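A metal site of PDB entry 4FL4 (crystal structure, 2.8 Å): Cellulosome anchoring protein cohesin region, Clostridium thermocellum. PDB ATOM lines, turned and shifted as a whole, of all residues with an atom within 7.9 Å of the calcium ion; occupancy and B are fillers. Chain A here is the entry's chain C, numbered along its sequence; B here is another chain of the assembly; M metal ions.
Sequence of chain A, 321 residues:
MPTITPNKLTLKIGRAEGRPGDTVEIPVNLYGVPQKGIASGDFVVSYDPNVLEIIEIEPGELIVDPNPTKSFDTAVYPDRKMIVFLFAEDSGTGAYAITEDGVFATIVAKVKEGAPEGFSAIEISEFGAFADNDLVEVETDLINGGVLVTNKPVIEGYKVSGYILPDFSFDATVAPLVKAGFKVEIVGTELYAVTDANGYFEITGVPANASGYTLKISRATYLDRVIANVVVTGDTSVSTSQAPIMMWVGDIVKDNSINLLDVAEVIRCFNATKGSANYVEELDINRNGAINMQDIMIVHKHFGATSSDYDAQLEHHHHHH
The calcium ion is bound by the side-chain amide oxygen (OD1) of Asn 286.
OD2 of Asp 295 binds the calcium ion, 2.5 Å away.
O of Ala 290 binds the calcium ion, at 2.6 Å.
The calcium ion is bound by OD1 of Asn 288, 2.6 Å away.
The side-chain carboxylate (OD1) of Asp 284 is bound to the calcium ion (2.6 Å).
OD1 of Asp 295 binds the calcium ion.
The calcium ion has six donor atoms within binding distance.
ND2 of Asn 286 is in hydrogen-bond range of OE1 of Gln 294 (3.1 Å).
The side-chain carboxylate (OD2) of Asp 295 sits close to the backbone NH (N) of Asn 292, at 3.1 Å.
OD1 of Asp 295 lies close to N of Ile 285 (3.1 Å).
OE1 of Gln 294 sits at hydrogen-bond distance from ND2 of Asn 288, 2.7 Å away.
The side-chain carboxylate (OD1) of Asp 284 sits close to the backbone NH (N) of Arg 287, 3.2 Å away.
The backbone NH (N) of Gly 289 sits at hydrogen-bond distance from the side-chain carboxylate (OD2) of Asp 284 (2.8 Å).
OH of Tyr 279 sits at hydrogen-bond distance from OD2 of Asp 284.
Five residues have an atom within 4 Å of the calcium ion: Asp 284, Asn 286, Asn 288, Ala 290 and Asp 295.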
ATOM      1  N   ALA A 272     -15.574  26.963  30.735  1.00  0.00           N
ATOM      2  CA  ALA A 272     -15.106  28.313  31.055  1.00  0.00           C
ATOM      3  C   ALA A 272     -16.160  29.034  31.880  1.00  0.00           C
ATOM      4  O   ALA A 272     -17.349  28.742  31.754  1.00  0.00           O
ATOM      5  CB  ALA A 272     -14.816  29.084  29.787  1.00  0.00           C
ATOM      6  N   TYR A 279     -13.509  32.136  28.353  1.00  0.00           N
ATOM      7  CA  TYR A 279     -14.915  32.576  28.349  1.00  0.00           C
ATOM      8  C   TYR A 279     -15.254  33.578  27.255  1.00  0.00           C
ATOM      9  O   TYR A 279     -14.426  34.403  26.879  1.00  0.00           O
ATOM     10  CB  TYR A 279     -15.313  33.169  29.699  1.00  0.00           C
ATOM     11  CG  TYR A 279     -16.817  33.393  29.892  1.00  0.00           C
ATOM     12  CD1 TYR A 279     -17.368  34.670  29.841  1.00  0.00           C
ATOM     13  CD2 TYR A 279     -17.661  32.325  30.174  1.00  0.00           C
ATOM     14  CE1 TYR A 279     -18.730  34.877  30.042  1.00  0.00           C
ATOM     15  CE2 TYR A 279     -19.024  32.527  30.388  1.00  0.00           C
ATOM     16  CZ  TYR A 279     -19.550  33.813  30.311  1.00  0.00           C
ATOM     17  OH  TYR A 279     -20.908  33.996  30.511  1.00  0.00           O
ATOM     18  N   GLU A 281     -18.880  35.605  26.178  1.00  0.00           N
ATOM     19  CA  GLU A 281     -20.272  35.793  26.536  1.00  0.00           C
ATOM     20  C   GLU A 281     -21.283  35.230  25.526  1.00  0.00           C
ATOM     21  O   GLU A 281     -22.214  34.514  25.891  1.00  0.00           O
ATOM     22  CB  GLU A 281     -20.547  37.261  26.813  1.00  0.00           C
ATOM     23  CG  GLU A 281     -21.929  37.517  27.376  1.00  0.00           C
ATOM     24  CD  GLU A 281     -21.918  38.609  28.425  1.00  0.00           C
ATOM     25  OE1 GLU A 281     -22.917  39.388  28.500  1.00  0.00           O
ATOM     26  OE2 GLU A 281     -20.929  38.695  29.190  1.00  0.00           O
ATOM     27  N   LEU A 283     -21.101  32.908  23.725  1.00  0.00           N
ATOM     28  CA  LEU A 283     -21.068  31.440  23.716  1.00  0.00           C
ATOM     29  C   LEU A 283     -21.748  30.858  24.951  1.00  0.00           C
ATOM     30  O   LEU A 283     -22.228  29.730  24.920  1.00  0.00           O
ATOM     31  CB  LEU A 283     -19.643  30.918  23.571  1.00  0.00           C
ATOM     32  CG  LEU A 283     -19.036  31.215  22.193  1.00  0.00           C
ATOM     33  CD1 LEU A 283     -17.701  30.515  22.034  1.00  0.00           C
ATOM     34  CD2 LEU A 283     -19.998  30.812  21.076  1.00  0.00           C
ATOM     35  N   ASP A 284     -21.792  31.622  26.024  1.00  0.00           N
ATOM     36  CA  ASP A 284     -22.649  31.275  27.140  1.00  0.00           C
ATOM     37  C   ASP A 284     -24.104  31.489  26.723  1.00  0.00           C
ATOM     38  O   ASP A 284     -24.737  32.464  27.146  1.00  0.00           O
ATOM     39  CB  ASP A 284     -22.302  32.157  28.332  1.00  0.00           C
ATOM     40  CG  ASP A 284     -23.085  31.816  29.566  1.00  0.00           C
ATOM     41  OD1 ASP A 284     -23.880  30.837  29.543  1.00  0.00           O
ATOM     42  OD2 ASP A 284     -22.892  32.539  30.574  1.00  0.00           O
ATOM     43  N   ILE A 285     -24.632  30.588  25.884  1.00  0.00           N
ATOM     44  CA  ILE A 285     -25.937  30.746  25.222  1.00  0.00           C
ATOM     45  C   ILE A 285     -27.056  31.291  26.117  1.00  0.00           C
ATOM     46  O   ILE A 285     -27.868  32.109  25.680  1.00  0.00           O
ATOM     47  CB  ILE A 285     -26.432  29.440  24.540  1.00  0.00           C
ATOM     48  CG1 ILE A 285     -25.971  29.363  23.099  1.00  0.00           C
ATOM     49  CG2 ILE A 285     -27.947  29.404  24.483  1.00  0.00           C
ATOM     50  CD1 ILE A 285     -24.523  29.506  22.928  1.00  0.00           C
ATOM     51  N   ASN A 286     -27.099  30.832  27.356  1.00  0.00           N
ATOM     52  CA  ASN A 286     -28.182  31.188  28.246  1.00  0.00           C
ATOM     53  C   ASN A 286     -27.719  32.140  29.340  1.00  0.00           C
ATOM     54  O   ASN A 286     -28.432  32.397  30.302  1.00  0.00           O
ATOM     55  CB  ASN A 286     -28.790  29.926  28.875  1.00  0.00           C
ATOM     56  CG  ASN A 286     -27.876  29.292  29.944  1.00  0.00           C
ATOM     57  OD1 ASN A 286     -26.678  29.599  30.046  1.00  0.00           O
ATOM     58  ND2 ASN A 286     -28.451  28.419  30.750  1.00  0.00           N
ATOM     59  N   ARG A 287     -26.503  32.641  29.189  1.00  0.00           N
ATOM     60  CA  ARG A 287     -25.993  33.690  30.058  1.00  0.00           C
ATOM     61  C   ARG A 287     -26.110  33.360  31.542  1.00  0.00           C
ATOM     62  O   ARG A 287     -26.461  34.228  32.338  1.00  0.00           O
ATOM     63  CB  ARG A 287     -26.732  34.990  29.796  1.00  0.00           C
ATOM     64  CG  ARG A 287     -26.583  35.524  28.392  1.00  0.00           C
ATOM     65  CD  ARG A 287     -25.186  36.087  28.143  1.00  0.00           C
ATOM     66  NE  ARG A 287     -25.163  36.954  26.965  1.00  0.00           N
ATOM     67  CZ  ARG A 287     -25.544  36.580  25.742  1.00  0.00           C
ATOM     68  NH1 ARG A 287     -25.984  35.333  25.527  1.00  0.00           N
ATOM     69  NH2 ARG A 287     -25.486  37.432  24.740  1.00  0.00           N
ATOM     70  N   ASN A 288     -25.814  32.109  31.892  1.00  0.00           N
ATOM     71  CA  ASN A 288     -25.878  31.674  33.290  1.00  0.00           C
ATOM     72  C   ASN A 288     -24.536  31.754  34.023  1.00  0.00           C
ATOM     73  O   ASN A 288     -24.442  31.444  35.217  1.00  0.00           O
ATOM     74  CB  ASN A 288     -26.456  30.259  33.400  1.00  0.00           C
ATOM     75  CG  ASN A 288     -25.502  29.222  32.878  1.00  0.00           C
ATOM     76  OD1 ASN A 288     -24.394  29.551  32.406  1.00  0.00           O
ATOM     77  ND2 ASN A 288     -25.904  27.945  32.955  1.00  0.00           N
ATOM     78  N   GLY A 289     -23.495  32.157  33.311  1.00  0.00           N
ATOM     79  CA  GLY A 289     -22.210  32.410  33.938  1.00  0.00           C
ATOM     80  C   GLY A 289     -21.137  31.414  33.557  1.00  0.00           C
ATOM     81  O   GLY A 289     -19.976  31.594  33.913  1.00  0.00           O
ATOM     82  N   ALA A 290     -21.533  30.375  32.825  1.00  0.00           N
ATOM     83  CA  ALA A 290     -20.583  29.338  32.408  1.00  0.00           C
ATOM     84  C   ALA A 290     -20.958  28.739  31.060  1.00  0.00           C
ATOM     85  O   ALA A 290     -22.109  28.827  30.620  1.00  0.00           O
ATOM     86  CB  ALA A 290     -20.495  28.248  33.467  1.00  0.00           C
ATOM     87  N   ILE A 291     -19.975  28.141  30.388  1.00  0.00           N
ATOM     88  CA  ILE A 291     -20.236  27.481  29.120  1.00  0.00           C
ATOM     89  C   ILE A 291     -20.116  25.957  29.283  1.00  0.00           C
ATOM     90  O   ILE A 291     -19.027  25.449  29.541  1.00  0.00           O
ATOM     91  CB  ILE A 291     -19.293  27.976  28.016  1.00  0.00           C
ATOM     92  CG1 ILE A 291     -19.445  29.484  27.832  1.00  0.00           C
ATOM     93  CG2 ILE A 291     -19.603  27.273  26.716  1.00  0.00           C
ATOM     94  CD1 ILE A 291     -18.322  30.100  27.034  1.00  0.00           C
ATOM     95  N   ASN A 292     -21.234  25.250  29.147  1.00  0.00           N
ATOM     96  CA  ASN A 292     -21.231  23.843  29.466  1.00  0.00           C
ATOM     97  C   ASN A 292     -22.193  23.033  28.633  1.00  0.00           C
ATOM     98  O   ASN A 292     -22.697  23.508  27.630  1.00  0.00           O
ATOM     99  CB  ASN A 292     -21.536  23.659  30.942  1.00  0.00           C
ATOM    100  CG  ASN A 292     -22.748  24.383  31.356  1.00  0.00           C
ATOM    101  OD1 ASN A 292     -23.736  24.395  30.626  1.00  0.00           O
ATOM    102  ND2 ASN A 292     -22.700  25.042  32.516  1.00  0.00           N
ATOM    103  N   MET A 293     -22.438  21.790  29.037  1.00  0.00           N
ATOM    104  CA  MET A 293     -23.240  20.874  28.218  1.00  0.00           C
ATOM    105  C   MET A 293     -24.664  21.419  27.988  1.00  0.00           C
ATOM    106  O   MET A 293     -25.290  21.155  26.965  1.00  0.00           O
ATOM    107  CB  MET A 293     -23.252  19.474  28.846  1.00  0.00           C
ATOM    108  CG  MET A 293     -24.051  18.432  28.088  1.00  0.00           C
ATOM    109  SD  MET A 293     -23.718  18.371  26.316  1.00  0.00           S
ATOM    110  CE  MET A 293     -22.864  16.812  26.131  1.00  0.00           C
ATOM    111  N   GLN A 294     -25.145  22.197  28.941  1.00  0.00           N
ATOM    112  CA  GLN A 294     -26.480  22.749  28.861  1.00  0.00           C
ATOM    113  C   GLN A 294     -26.620  23.780  27.726  1.00  0.00           C
ATOM    114  O   GLN A 294     -27.666  23.855  27.061  1.00  0.00           O
ATOM    115  CB  GLN A 294     -26.851  23.366  30.190  1.00  0.00           C
ATOM    116  CG  GLN A 294     -27.966  24.337  30.110  1.00  0.00           C
ATOM    117  CD  GLN A 294     -28.119  25.112  31.385  1.00  0.00           C
ATOM    118  OE1 GLN A 294     -27.168  25.774  31.843  1.00  0.00           O
ATOM    119  NE2 GLN A 294     -29.307  25.026  31.986  1.00  0.00           N
ATOM    120  N   ASP A 295     -25.573  24.560  27.502  1.00  0.00           N
ATOM    121  CA  ASP A 295     -25.481  25.412  26.328  1.00  0.00           C
ATOM    122  C   ASP A 295     -25.509  24.583  25.041  1.00  0.00           C
ATOM    123  O   ASP A 295     -26.231  24.901  24.094  1.00  0.00           O
ATOM    124  CB  ASP A 295     -24.204  26.240  26.356  1.00  0.00           C
ATOM    125  CG  ASP A 295     -24.221  27.281  27.446  1.00  0.00           C
ATOM    126  OD1 ASP A 295     -25.227  28.012  27.571  1.00  0.00           O
ATOM    127  OD2 ASP A 295     -23.236  27.358  28.201  1.00  0.00           O
ATOM    128  N   ILE A 296     -24.716  23.517  25.006  1.00  0.00           N
ATOM    129  CA  ILE A 296     -24.577  22.738  23.796  1.00  0.00           C
ATOM    130  C   ILE A 296     -25.905  22.086  23.499  1.00  0.00           C
ATOM    131  O   ILE A 296     -26.260  21.854  22.341  1.00  0.00           O
ATOM    132  CB  ILE A 296     -23.477  21.654  23.971  1.00  0.00           C
ATOM    133  CG1 ILE A 296     -22.142  22.318  24.303  1.00  0.00           C
ATOM    134  CG2 ILE A 296     -23.358  20.741  22.743  1.00  0.00           C
ATOM    135  CD1 ILE A 296     -20.985  21.387  24.129  1.00  0.00           C
ATOM    136  N   ILE A 298     -28.802  23.361  24.056  1.00  0.00           N
ATOM    137  CA  ILE A 298     -29.640  24.360  23.420  1.00  0.00           C
ATOM    138  C   ILE A 298     -29.409  24.328  21.917  1.00  0.00           C
ATOM    139  O   ILE A 298     -30.347  24.150  21.129  1.00  0.00           O
ATOM    140  CB  ILE A 298     -29.372  25.741  24.005  1.00  0.00           C
ATOM    141  CG1 ILE A 298     -30.062  25.850  25.365  1.00  0.00           C
ATOM    142  CG2 ILE A 298     -29.865  26.831  23.049  1.00  0.00           C
ATOM    143  CD1 ILE A 298     -29.541  26.935  26.202  1.00  0.00           C
ATOM    144  N   SER B 151     -18.334  25.653  37.222  1.00  0.00           N
ATOM    145  CA  SER B 151     -18.606  25.309  35.841  1.00  0.00           C
ATOM    146  C   SER B 151     -20.034  24.826  35.607  1.00  0.00           C
ATOM    147  O   SER B 151     -20.459  24.736  34.467  1.00  0.00           O
ATOM    148  CB  SER B 151     -17.639  24.231  35.366  1.00  0.00           C
ATOM    149  OG  SER B 151     -16.364  24.786  35.094  1.00  0.00           O
ATOM    150  N   PRO B 153     -23.436  26.049  37.122  1.00  0.00           N
ATOM    151  CA  PRO B 153     -24.421  26.760  37.940  1.00  0.00           C
ATOM    152  C   PRO B 153     -25.813  26.209  37.690  1.00  0.00           C
ATOM    153  O   PRO B 153     -26.161  25.907  36.538  1.00  0.00           O
ATOM    154  CB  PRO B 153     -24.335  28.199  37.441  1.00  0.00           C
ATOM    155  CG  PRO B 153     -23.095  28.280  36.608  1.00  0.00           C
ATOM    156  CD  PRO B 153     -22.893  26.911  36.056  1.00  0.00           C
ATOM    157  N   GLN B 160     -26.177  17.426  35.966  1.00  0.00           N
ATOM    158  CA  GLN B 160     -27.181  18.019  35.103  1.00  0.00           C
ATOM    159  C   GLN B 160     -27.602  16.996  34.068  1.00  0.00           C
ATOM    160  O   GLN B 160     -26.763  16.455  33.349  1.00  0.00           O
ATOM    161  CB  GLN B 160     -26.694  19.322  34.468  1.00  0.00           C
ATOM    162  CG  GLN B 160     -27.587  20.535  34.800  1.00  0.00           C
ATOM    163  CD  GLN B 160     -26.962  21.880  34.457  1.00  0.00           C
ATOM    164  OE1 GLN B 160     -25.907  21.969  33.799  1.00  0.00           O
ATOM    165  NE2 GLN B 160     -27.621  22.949  34.890  1.00  0.00           N
HETATM  166 CA    CA M   1     -24.569  28.365  30.114  1.00  0.00          CA
